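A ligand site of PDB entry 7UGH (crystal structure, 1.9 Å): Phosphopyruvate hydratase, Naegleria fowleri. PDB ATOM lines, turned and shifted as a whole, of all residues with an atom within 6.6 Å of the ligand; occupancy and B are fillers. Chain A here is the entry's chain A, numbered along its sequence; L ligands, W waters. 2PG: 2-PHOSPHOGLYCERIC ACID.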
ATOM      1  N   ARG A  59      -8.403 -33.717  18.027  1.00  0.00           N
ATOM      2  CA  ARG A  59      -8.800 -35.098  17.843  1.00  0.00           C
ATOM      3  C   ARG A  59      -7.727 -36.074  18.292  1.00  0.00           C
ATOM      4  O   ARG A  59      -7.917 -37.290  18.158  1.00  0.00           O
ATOM      5  CB  ARG A  59      -9.136 -35.398  16.375  1.00  0.00           C
ATOM      6  CG  ARG A  59     -10.483 -34.952  15.960  1.00  0.00           C
ATOM      7  CD  ARG A  59     -10.891 -35.714  14.718  1.00  0.00           C
ATOM      8  NE  ARG A  59     -10.262 -35.097  13.576  1.00  0.00           N
ATOM      9  CZ  ARG A  59     -10.746 -35.172  12.345  1.00  0.00           C
ATOM     10  NH1 ARG A  59     -11.826 -35.909  12.080  1.00  0.00           N
ATOM     11  NH2 ARG A  59     -10.159 -34.491  11.367  1.00  0.00           N
ATOM     12  N   SER A  84      -6.639 -29.248  10.996  1.00  0.00           N
ATOM     13  CA  SER A  84      -6.640 -30.334  10.011  1.00  0.00           C
ATOM     14  C   SER A  84      -8.045 -30.883   9.804  1.00  0.00           C
ATOM     15  O   SER A  84      -8.706 -31.283  10.766  1.00  0.00           O
ATOM     16  CB  SER A  84      -5.745 -31.486  10.463  1.00  0.00           C
ATOM     17  OG  SER A  84      -5.831 -32.581   9.553  1.00  0.00           O
ATOM     18  N   GLY A  85      -8.479 -30.966   8.535  1.00  0.00           N
ATOM     19  CA  GLY A  85      -9.773 -31.543   8.232  1.00  0.00           C
ATOM     20  C   GLY A  85      -9.753 -33.050   8.280  1.00  0.00           C
ATOM     21  O   GLY A  85      -8.702 -33.679   8.391  1.00  0.00           O
ATOM     22  N   ALA A  86     -10.953 -33.632   8.232  1.00  0.00           N
ATOM     23  CA  ALA A  86     -11.054 -35.088   8.244  1.00  0.00           C
ATOM     24  C   ALA A  86     -10.566 -35.696   6.929  1.00  0.00           C
ATOM     25  O   ALA A  86     -10.234 -36.885   6.907  1.00  0.00           O
ATOM     26  CB  ALA A  86     -12.497 -35.501   8.541  1.00  0.00           C
ATOM     27  N   SER A  87     -10.492 -34.909   5.860  1.00  0.00           N
ATOM     28  CA  SER A  87     -10.043 -35.398   4.563  1.00  0.00           C
ATOM     29  C   SER A  87      -9.413 -34.239   3.797  1.00  0.00           C
ATOM     30  O   SER A  87      -9.779 -33.076   3.985  1.00  0.00           O
ATOM     31  CB  SER A  87     -11.205 -36.003   3.754  1.00  0.00           C
ATOM     32  OG  SER A  87     -10.778 -36.433   2.472  1.00  0.00           O
ATOM     33  N   LYS A 208     -22.240 -39.641   8.482  1.00  0.00           N
ATOM     34  CA  LYS A 208     -21.138 -40.466   8.984  1.00  0.00           C
ATOM     35  C   LYS A 208     -20.962 -40.369  10.496  1.00  0.00           C
ATOM     36  O   LYS A 208     -20.340 -41.261  11.090  1.00  0.00           O
ATOM     37  CB  LYS A 208     -19.819 -40.061   8.305  1.00  0.00           C
ATOM     38  CG  LYS A 208     -19.249 -38.717   8.798  1.00  0.00           C
ATOM     39  CD  LYS A 208     -18.087 -38.211   7.924  1.00  0.00           C
ATOM     40  CE  LYS A 208     -17.504 -36.894   8.471  1.00  0.00           C
ATOM     41  NZ  LYS A 208     -16.325 -36.353   7.702  1.00  0.00           N
ATOM     42  N   GLN A 217     -25.434 -33.978   7.389  1.00  0.00           N
ATOM     43  CA  GLN A 217     -24.335 -34.165   8.334  1.00  0.00           C
ATOM     44  C   GLN A 217     -24.425 -33.240   9.543  1.00  0.00           C
ATOM     45  O   GLN A 217     -24.129 -33.672  10.668  1.00  0.00           O
ATOM     46  CB  GLN A 217     -22.993 -33.988   7.616  1.00  0.00           C
ATOM     47  CG  GLN A 217     -21.791 -34.274   8.498  1.00  0.00           C
ATOM     48  CD  GLN A 217     -20.491 -34.345   7.698  1.00  0.00           C
ATOM     49  OE1 GLN A 217     -20.158 -35.387   7.134  1.00  0.00           O
ATOM     50  NE2 GLN A 217     -19.767 -33.240   7.630  1.00  0.00           N
ATOM     51  N   GLU A 218     -24.793 -31.979   9.359  1.00  0.00           N
ATOM     52  CA  GLU A 218     -24.718 -31.021  10.455  1.00  0.00           C
ATOM     53  C   GLU A 218     -25.976 -30.175  10.519  1.00  0.00           C
ATOM     54  O   GLU A 218     -26.454 -29.670   9.502  1.00  0.00           O
ATOM     55  CB  GLU A 218     -23.515 -30.063  10.332  1.00  0.00           C
ATOM     56  CG  GLU A 218     -22.187 -30.747  10.161  1.00  0.00           C
ATOM     57  CD  GLU A 218     -21.053 -29.732   9.990  1.00  0.00           C
ATOM     58  OE1 GLU A 218     -21.332 -28.513   9.898  1.00  0.00           O
ATOM     59  OE2 GLU A 218     -19.881 -30.170   9.934  1.00  0.00           O
ATOM     60  N   GLU A 261     -16.781 -31.888  16.885  1.00  0.00           N
ATOM     61  CA  GLU A 261     -17.000 -30.449  16.970  1.00  0.00           C
ATOM     62  C   GLU A 261     -17.947 -30.090  18.093  1.00  0.00           C
ATOM     63  O   GLU A 261     -18.381 -28.928  18.157  1.00  0.00           O
ATOM     64  CB  GLU A 261     -17.533 -29.888  15.649  1.00  0.00           C
ATOM     65  CG  GLU A 261     -16.677 -30.217  14.442  1.00  0.00           C
ATOM     66  CD  GLU A 261     -17.239 -31.371  13.627  1.00  0.00           C
ATOM     67  OE1 GLU A 261     -18.345 -31.877  13.949  1.00  0.00           O
ATOM     68  OE2 GLU A 261     -16.559 -31.791  12.659  1.00  0.00           O
ATOM     69  N   ASP A 298     -25.575 -28.183   7.082  1.00  0.00           N
ATOM     70  CA  ASP A 298     -24.464 -28.587   6.225  1.00  0.00           C
ATOM     71  C   ASP A 298     -24.767 -30.038   5.871  1.00  0.00           C
ATOM     72  O   ASP A 298     -24.602 -30.921   6.708  1.00  0.00           O
ATOM     73  CB  ASP A 298     -23.101 -28.449   6.908  1.00  0.00           C
ATOM     74  CG  ASP A 298     -21.949 -29.026   6.079  1.00  0.00           C
ATOM     75  OD1 ASP A 298     -22.164 -29.417   4.907  1.00  0.00           O
ATOM     76  OD2 ASP A 298     -20.827 -29.101   6.596  1.00  0.00           O
ATOM     77  N   ALA A 300     -23.256 -31.914   3.675  1.00  0.00           N
ATOM     78  CA  ALA A 300     -22.103 -32.668   3.180  1.00  0.00           C
ATOM     79  C   ALA A 300     -22.558 -33.715   2.163  1.00  0.00           C
ATOM     80  O   ALA A 300     -22.281 -34.912   2.263  1.00  0.00           O
ATOM     81  CB  ALA A 300     -21.329 -33.300   4.343  1.00  0.00           C
ATOM     82  N   GLU A 344     -25.582 -25.547   3.507  1.00  0.00           N
ATOM     83  CA  GLU A 344     -24.209 -25.703   3.051  1.00  0.00           C
ATOM     84  C   GLU A 344     -24.048 -27.045   2.360  1.00  0.00           C
ATOM     85  O   GLU A 344     -24.550 -28.065   2.841  1.00  0.00           O
ATOM     86  CB  GLU A 344     -23.237 -25.597   4.240  1.00  0.00           C
ATOM     87  CG  GLU A 344     -21.772 -25.925   3.918  1.00  0.00           C
ATOM     88  CD  GLU A 344     -20.899 -25.908   5.171  1.00  0.00           C
ATOM     89  OE1 GLU A 344     -21.278 -25.233   6.171  1.00  0.00           O
ATOM     90  OE2 GLU A 344     -19.856 -26.605   5.164  1.00  0.00           O
ATOM     91  N   ASP A 345     -23.354 -27.038   1.213  1.00  0.00           N
ATOM     92  CA  ASP A 345     -23.092 -28.255   0.437  1.00  0.00           C
ATOM     93  C   ASP A 345     -24.346 -29.116   0.268  1.00  0.00           C
ATOM     94  O   ASP A 345     -24.326 -30.335   0.434  1.00  0.00           O
ATOM     95  CB  ASP A 345     -21.955 -29.077   1.060  1.00  0.00           C
ATOM     96  CG  ASP A 345     -20.568 -28.535   0.670  1.00  0.00           C
ATOM     97  OD1 ASP A 345     -20.500 -27.677  -0.232  1.00  0.00           O
ATOM     98  OD2 ASP A 345     -19.571 -28.987   1.271  1.00  0.00           O
ATOM     99  N   ASP A 371     -18.911 -25.315   0.310  1.00  0.00           N
ATOM    100  CA  ASP A 371     -17.737 -25.748   1.074  1.00  0.00           C
ATOM    101  C   ASP A 371     -16.902 -26.657   0.193  1.00  0.00           C
ATOM    102  O   ASP A 371     -15.919 -26.203  -0.417  1.00  0.00           O
ATOM    103  CB  ASP A 371     -18.135 -26.461   2.370  1.00  0.00           C
ATOM    104  CG  ASP A 371     -16.939 -27.059   3.107  1.00  0.00           C
ATOM    105  OD1 ASP A 371     -15.791 -26.625   2.890  1.00  0.00           O
ATOM    106  OD2 ASP A 371     -17.134 -28.001   3.908  1.00  0.00           O
ATOM    107  N   ASP A 372     -17.284 -27.945   0.102  1.00  0.00           N
ATOM    108  CA  ASP A 372     -16.647 -28.822  -0.887  1.00  0.00           C
ATOM    109  C   ASP A 372     -16.789 -28.282  -2.294  1.00  0.00           C
ATOM    110  O   ASP A 372     -15.955 -28.596  -3.162  1.00  0.00           O
ATOM    111  CB  ASP A 372     -17.264 -30.232  -0.843  1.00  0.00           C
ATOM    112  CG  ASP A 372     -17.044 -30.926   0.501  1.00  0.00           C
ATOM    113  OD1 ASP A 372     -16.160 -30.518   1.269  1.00  0.00           O
ATOM    114  OD2 ASP A 372     -17.776 -31.885   0.794  1.00  0.00           O
ATOM    115  N   LEU A 394     -17.657 -21.012   2.317  1.00  0.00           N
ATOM    116  CA  LEU A 394     -17.057 -21.442   3.575  1.00  0.00           C
ATOM    117  C   LEU A 394     -15.528 -21.365   3.425  1.00  0.00           C
ATOM    118  O   LEU A 394     -14.949 -22.090   2.613  1.00  0.00           O
ATOM    119  CB  LEU A 394     -17.503 -22.866   3.937  1.00  0.00           C
ATOM    120  CG  LEU A 394     -17.195 -23.259   5.389  1.00  0.00           C
ATOM    121  CD1 LEU A 394     -18.215 -22.592   6.330  1.00  0.00           C
ATOM    122  CD2 LEU A 394     -17.206 -24.795   5.611  1.00  0.00           C
ATOM    123  N   LYS A 396     -11.803 -21.846   4.504  1.00  0.00           N
ATOM    124  CA  LYS A 396     -10.898 -22.598   5.370  1.00  0.00           C
ATOM    125  C   LYS A 396      -9.474 -22.212   4.982  1.00  0.00           C
ATOM    126  O   LYS A 396      -8.991 -22.629   3.929  1.00  0.00           O
ATOM    127  CB  LYS A 396     -11.111 -24.112   5.242  1.00  0.00           C
ATOM    128  CG  LYS A 396     -12.457 -24.574   5.833  1.00  0.00           C
ATOM    129  CD  LYS A 396     -12.916 -25.911   5.277  1.00  0.00           C
ATOM    130  CE  LYS A 396     -14.129 -26.493   6.042  1.00  0.00           C
ATOM    131  NZ  LYS A 396     -14.570 -27.783   5.442  1.00  0.00           N
ATOM    132  N   ASN A 398      -6.610 -23.177   5.817  1.00  0.00           N
ATOM    133  CA  ASN A 398      -5.627 -24.235   5.586  1.00  0.00           C
ATOM    134  C   ASN A 398      -5.939 -25.040   4.336  1.00  0.00           C
ATOM    135  O   ASN A 398      -5.054 -25.757   3.865  1.00  0.00           O
ATOM    136  CB  ASN A 398      -5.481 -25.140   6.827  1.00  0.00           C
ATOM    137  CG  ASN A 398      -6.501 -26.255   6.877  1.00  0.00           C
ATOM    138  OD1 ASN A 398      -7.697 -26.016   6.982  1.00  0.00           O
ATOM    139  ND2 ASN A 398      -6.030 -27.484   6.812  1.00  0.00           N
ATOM    140  N   GLN A 399      -7.126 -24.904   3.749  1.00  0.00           N
ATOM    141  CA  GLN A 399      -7.372 -25.502   2.440  1.00  0.00           C
ATOM    142  C   GLN A 399      -6.597 -24.805   1.336  1.00  0.00           C
ATOM    143  O   GLN A 399      -6.270 -25.433   0.312  1.00  0.00           O
ATOM    144  CB  GLN A 399      -8.848 -25.459   2.090  1.00  0.00           C
ATOM    145  CG  GLN A 399      -9.613 -26.642   2.602  1.00  0.00           C
ATOM    146  CD  GLN A 399     -11.027 -26.656   2.073  1.00  0.00           C
ATOM    147  OE1 GLN A 399     -11.637 -25.601   1.836  1.00  0.00           O
ATOM    148  NE2 GLN A 399     -11.563 -27.870   1.898  1.00  0.00           N
ATOM    149  N   SER A 423     -14.294 -20.591   8.728  1.00  0.00           N
ATOM    150  CA  SER A 423     -14.638 -21.910   9.227  1.00  0.00           C
ATOM    151  C   SER A 423     -13.502 -22.515  10.043  1.00  0.00           C
ATOM    152  O   SER A 423     -12.318 -22.325   9.746  1.00  0.00           O
ATOM    153  CB  SER A 423     -14.980 -22.866   8.066  1.00  0.00           C
ATOM    154  OG  SER A 423     -15.361 -24.135   8.548  1.00  0.00           O
ATOM    155  N   HIS A 424     -13.889 -23.306  11.048  1.00  0.00           N
ATOM    156  CA  HIS A 424     -12.989 -24.247  11.710  1.00  0.00           C
ATOM    157  C   HIS A 424     -12.727 -25.459  10.815  1.00  0.00           C
ATOM    158  O   HIS A 424     -13.322 -25.640   9.745  1.00  0.00           O
ATOM    159  CB  HIS A 424     -13.585 -24.712  13.036  1.00  0.00           C
ATOM    160  CG  HIS A 424     -14.900 -25.454  12.914  1.00  0.00           C
ATOM    161  ND1 HIS A 424     -15.526 -26.045  13.988  1.00  0.00           N
ATOM    162  CD2 HIS A 424     -15.699 -25.691  11.839  1.00  0.00           C
ATOM    163  CE1 HIS A 424     -16.645 -26.619  13.592  1.00  0.00           C
ATOM    164  NE2 HIS A 424     -16.780 -26.410  12.291  1.00  0.00           N
ATOM    165  N   ARG A 425     -11.834 -26.340  11.270  1.00  0.00           N
ATOM    166  CA  ARG A 425     -11.743 -27.699  10.758  1.00  0.00           C
ATOM    167  C   ARG A 425     -12.121 -28.678  11.860  1.00  0.00           C
ATOM    168  O   ARG A 425     -12.134 -28.340  13.048  1.00  0.00           O
ATOM    169  CB  ARG A 425     -10.334 -28.011  10.217  1.00  0.00           C
ATOM    170  CG  ARG A 425      -9.791 -26.990   9.201  1.00  0.00           C
ATOM    171  CD  ARG A 425     -10.681 -26.885   7.961  1.00  0.00           C
ATOM    172  NE  ARG A 425     -10.918 -28.172   7.315  1.00  0.00           N
ATOM    173  CZ  ARG A 425     -10.234 -28.629   6.267  1.00  0.00           C
ATOM    174  NH1 ARG A 425      -9.197 -27.985   5.782  1.00  0.00           N
ATOM    175  NH2 ARG A 425     -10.614 -29.775   5.698  1.00  0.00           N
ATOM    176  N   SER A 426     -12.370 -29.928  11.448  1.00  0.00           N
ATOM    177  CA  SER A 426     -12.766 -30.928  12.430  1.00  0.00           C
ATOM    178  C   SER A 426     -11.649 -31.212  13.435  1.00  0.00           C
ATOM    179  O   SER A 426     -11.928 -31.501  14.598  1.00  0.00           O
ATOM    180  CB  SER A 426     -13.222 -32.211  11.727  1.00  0.00           C
ATOM    181  OG  SER A 426     -12.218 -32.741  10.880  1.00  0.00           O
ATOM    182  N   GLY A 427     -10.386 -31.112  13.030  1.00  0.00           N
ATOM    183  CA  GLY A 427      -9.300 -31.143  13.977  1.00  0.00           C
ATOM    184  C   GLY A 427      -8.809 -29.718  14.203  1.00  0.00           C
ATOM    185  O   GLY A 427      -8.245 -29.101  13.297  1.00  0.00           O
ATOM    186  N   LYS A 447     -18.141 -20.190  11.602  1.00  0.00           N
ATOM    187  CA  LYS A 447     -18.624 -21.548  11.876  1.00  0.00           C
ATOM    188  C   LYS A 447     -17.502 -22.244  12.633  1.00  0.00           C
ATOM    189  O   LYS A 447     -16.495 -22.647  12.025  1.00  0.00           O
ATOM    190  CB  LYS A 447     -18.956 -22.281  10.579  1.00  0.00           C
ATOM    191  CG  LYS A 447     -19.615 -23.644  10.771  1.00  0.00           C
ATOM    192  CD  LYS A 447     -19.592 -24.359   9.411  1.00  0.00           C
ATOM    193  CE  LYS A 447     -20.145 -25.732   9.482  1.00  0.00           C
ATOM    194  NZ  LYS A 447     -19.837 -26.447   8.205  1.00  0.00           N
ATOM    195  N   ARG A 456     -13.347 -25.274  20.428  1.00  0.00           N
ATOM    196  CA  ARG A 456     -14.484 -24.538  19.896  1.00  0.00           C
ATOM    197  C   ARG A 456     -14.810 -23.345  20.781  1.00  0.00           C
ATOM    198  O   ARG A 456     -14.892 -22.210  20.277  1.00  0.00           O
ATOM    199  CB  ARG A 456     -15.737 -25.439  19.757  1.00  0.00           C
ATOM    200  CG  ARG A 456     -15.449 -26.831  19.177  1.00  0.00           C
ATOM    201  CD  ARG A 456     -14.767 -26.816  17.785  1.00  0.00           C
ATOM    202  NE  ARG A 456     -14.218 -28.142  17.501  1.00  0.00           N
ATOM    203  CZ  ARG A 456     -13.586 -28.501  16.392  1.00  0.00           C
ATOM    204  NH1 ARG A 456     -13.627 -27.744  15.302  1.00  0.00           N
ATOM    205  NH2 ARG A 456     -12.865 -29.627  16.389  1.00  0.00           N
HETATM  206  C1  2PG L   1     -16.821 -28.704   7.440  1.00  0.00           C
HETATM  207  C2  2PG L   1     -15.647 -28.896   8.383  1.00  0.00           C
HETATM  208  C3  2PG L   1     -16.116 -28.815   9.833  1.00  0.00           C
HETATM  209  P   2PG L   1     -13.670 -30.792   7.850  1.00  0.00           P
HETATM  210  O1  2PG L   1     -17.412 -27.651   7.370  1.00  0.00           O
HETATM  211  O2  2PG L   1     -17.129 -29.773   6.712  1.00  0.00           O
HETATM  212  O3  2PG L   1     -17.526 -28.607   9.979  1.00  0.00           O
HETATM  213  O1P 2PG L   1     -15.162 -30.263   8.192  1.00  0.00           O
HETATM  214  O2P 2PG L   1     -13.535 -32.224   8.240  1.00  0.00           O
HETATM  215  O3P 2PG L   1     -13.467 -30.590   6.341  1.00  0.00           O
HETATM  216  O4P 2PG L   1     -12.703 -29.880   8.566  1.00  0.00           O
HETATM  217  O   HOH W   1     -17.050 -32.667   6.651  1.00  0.00           O
HETATM  218  O   HOH W   2     -12.618 -32.823   5.570  1.00  0.00           O
HETATM  219  O   HOH W   3     -16.340 -30.281   3.989  1.00  0.00           O
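An oxygen (O1) of the ligand sits close to the side-chain carboxylate of Glu 344 (3.5 Å). O2 of the ligand sits close to OD2 of Asp 371, 3.3 Å away. Gly 85 touches the ligand (CA to O4P, 3.4 Å). OD2 of Asp 298 touches O2 of the ligand (3.8 Å). Leu 394 touches the ligand. Within 4 Å of the ligand: Gly 85, Ala 86, Glu 218, Asp 298, Glu 344, Asp 371, Leu 394, Lys 396, His 424, Arg 425, Ser 426 and Lys 447. The nearest printed residue that does not touch the ligand is Glu 261 (4.1 Å).
An oxygen (O4P) of the ligand lies within salt-bridge range of the guanidinium group (NE) of Arg 425 (2.8 Å). The side-chain carboxylate (OE2) of Glu 218 sits at hydrogen-bond distance from an oxygen (O3) of the ligand (2.8 Å). NZ of Lys 447 is in salt-bridge range of O1 of the ligand, at 2.8 Å. N of Ser 426 is in hydrogen-bond range of O4P of the ligand, at 2.9 Å. The side-chain hydroxyl of Ser 426 lies within hydrogen-bond range of an oxygen (O2P) of the ligand (3.0 Å). An oxygen (O2P) of the ligand lies within hydrogen-bond range of the backbone NH of Ala 86, 2.9 Å away. O3P of the ligand lies within salt-bridge range of NZ of Lys 396, 3.1 Å away. A ring nitrogen (NE2) of His 424 is in hydrogen-bond range of an oxygen (O3) of the ligand (3.3 Å).
Water W2 lies within hydrogen-bond range of O3P of the ligand (2.5 Å), N of Ser 87 (3.0 Å) and N of Ala 86 (3.2 Å). Water W3 lies within hydrogen-bond range of OD2 of Asp 371 (2.4 Å), OD1 of Asp 372 (2.7 Å), O2 of the ligand (2.9 Å) and NZ of Lys 396 (3.4 Å). Water W1 bridges an oxygen (O2) of the ligand (2.9 Å) and the side-chain amide nitrogen (NE2) of Gln 217 (2.9 Å).
NZ of Lys 447 is in salt-bridge range of OE1 of Glu 218 (3.1 Å). N of Glu 218 lies within hydrogen-bond range of O of Asp 298 (2.9 Å). The backbone NH of Ala 86 lies within hydrogen-bond range of the side-chain hydroxyl of Ser 426 (3.1 Å). The backbone carbonyl oxygen (O) of Ser 426 is in hydrogen-bond range of the guanidinium group (NH2) of Arg 456 (2.8 Å). OD1 of Asp 345 lies within hydrogen-bond range of N of Asp 371, at 2.9 Å. NH2 of Arg 59 sits at hydrogen-bond distance from O of Gly 85, at 3.4 Å. O of Asp 298 is in hydrogen-bond range of N of Gln 217 (3.2 Å). The side-chain carboxylate of Asp 298 is in hydrogen-bond range of the backbone NH of Ala 300, 3.0 Å away.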
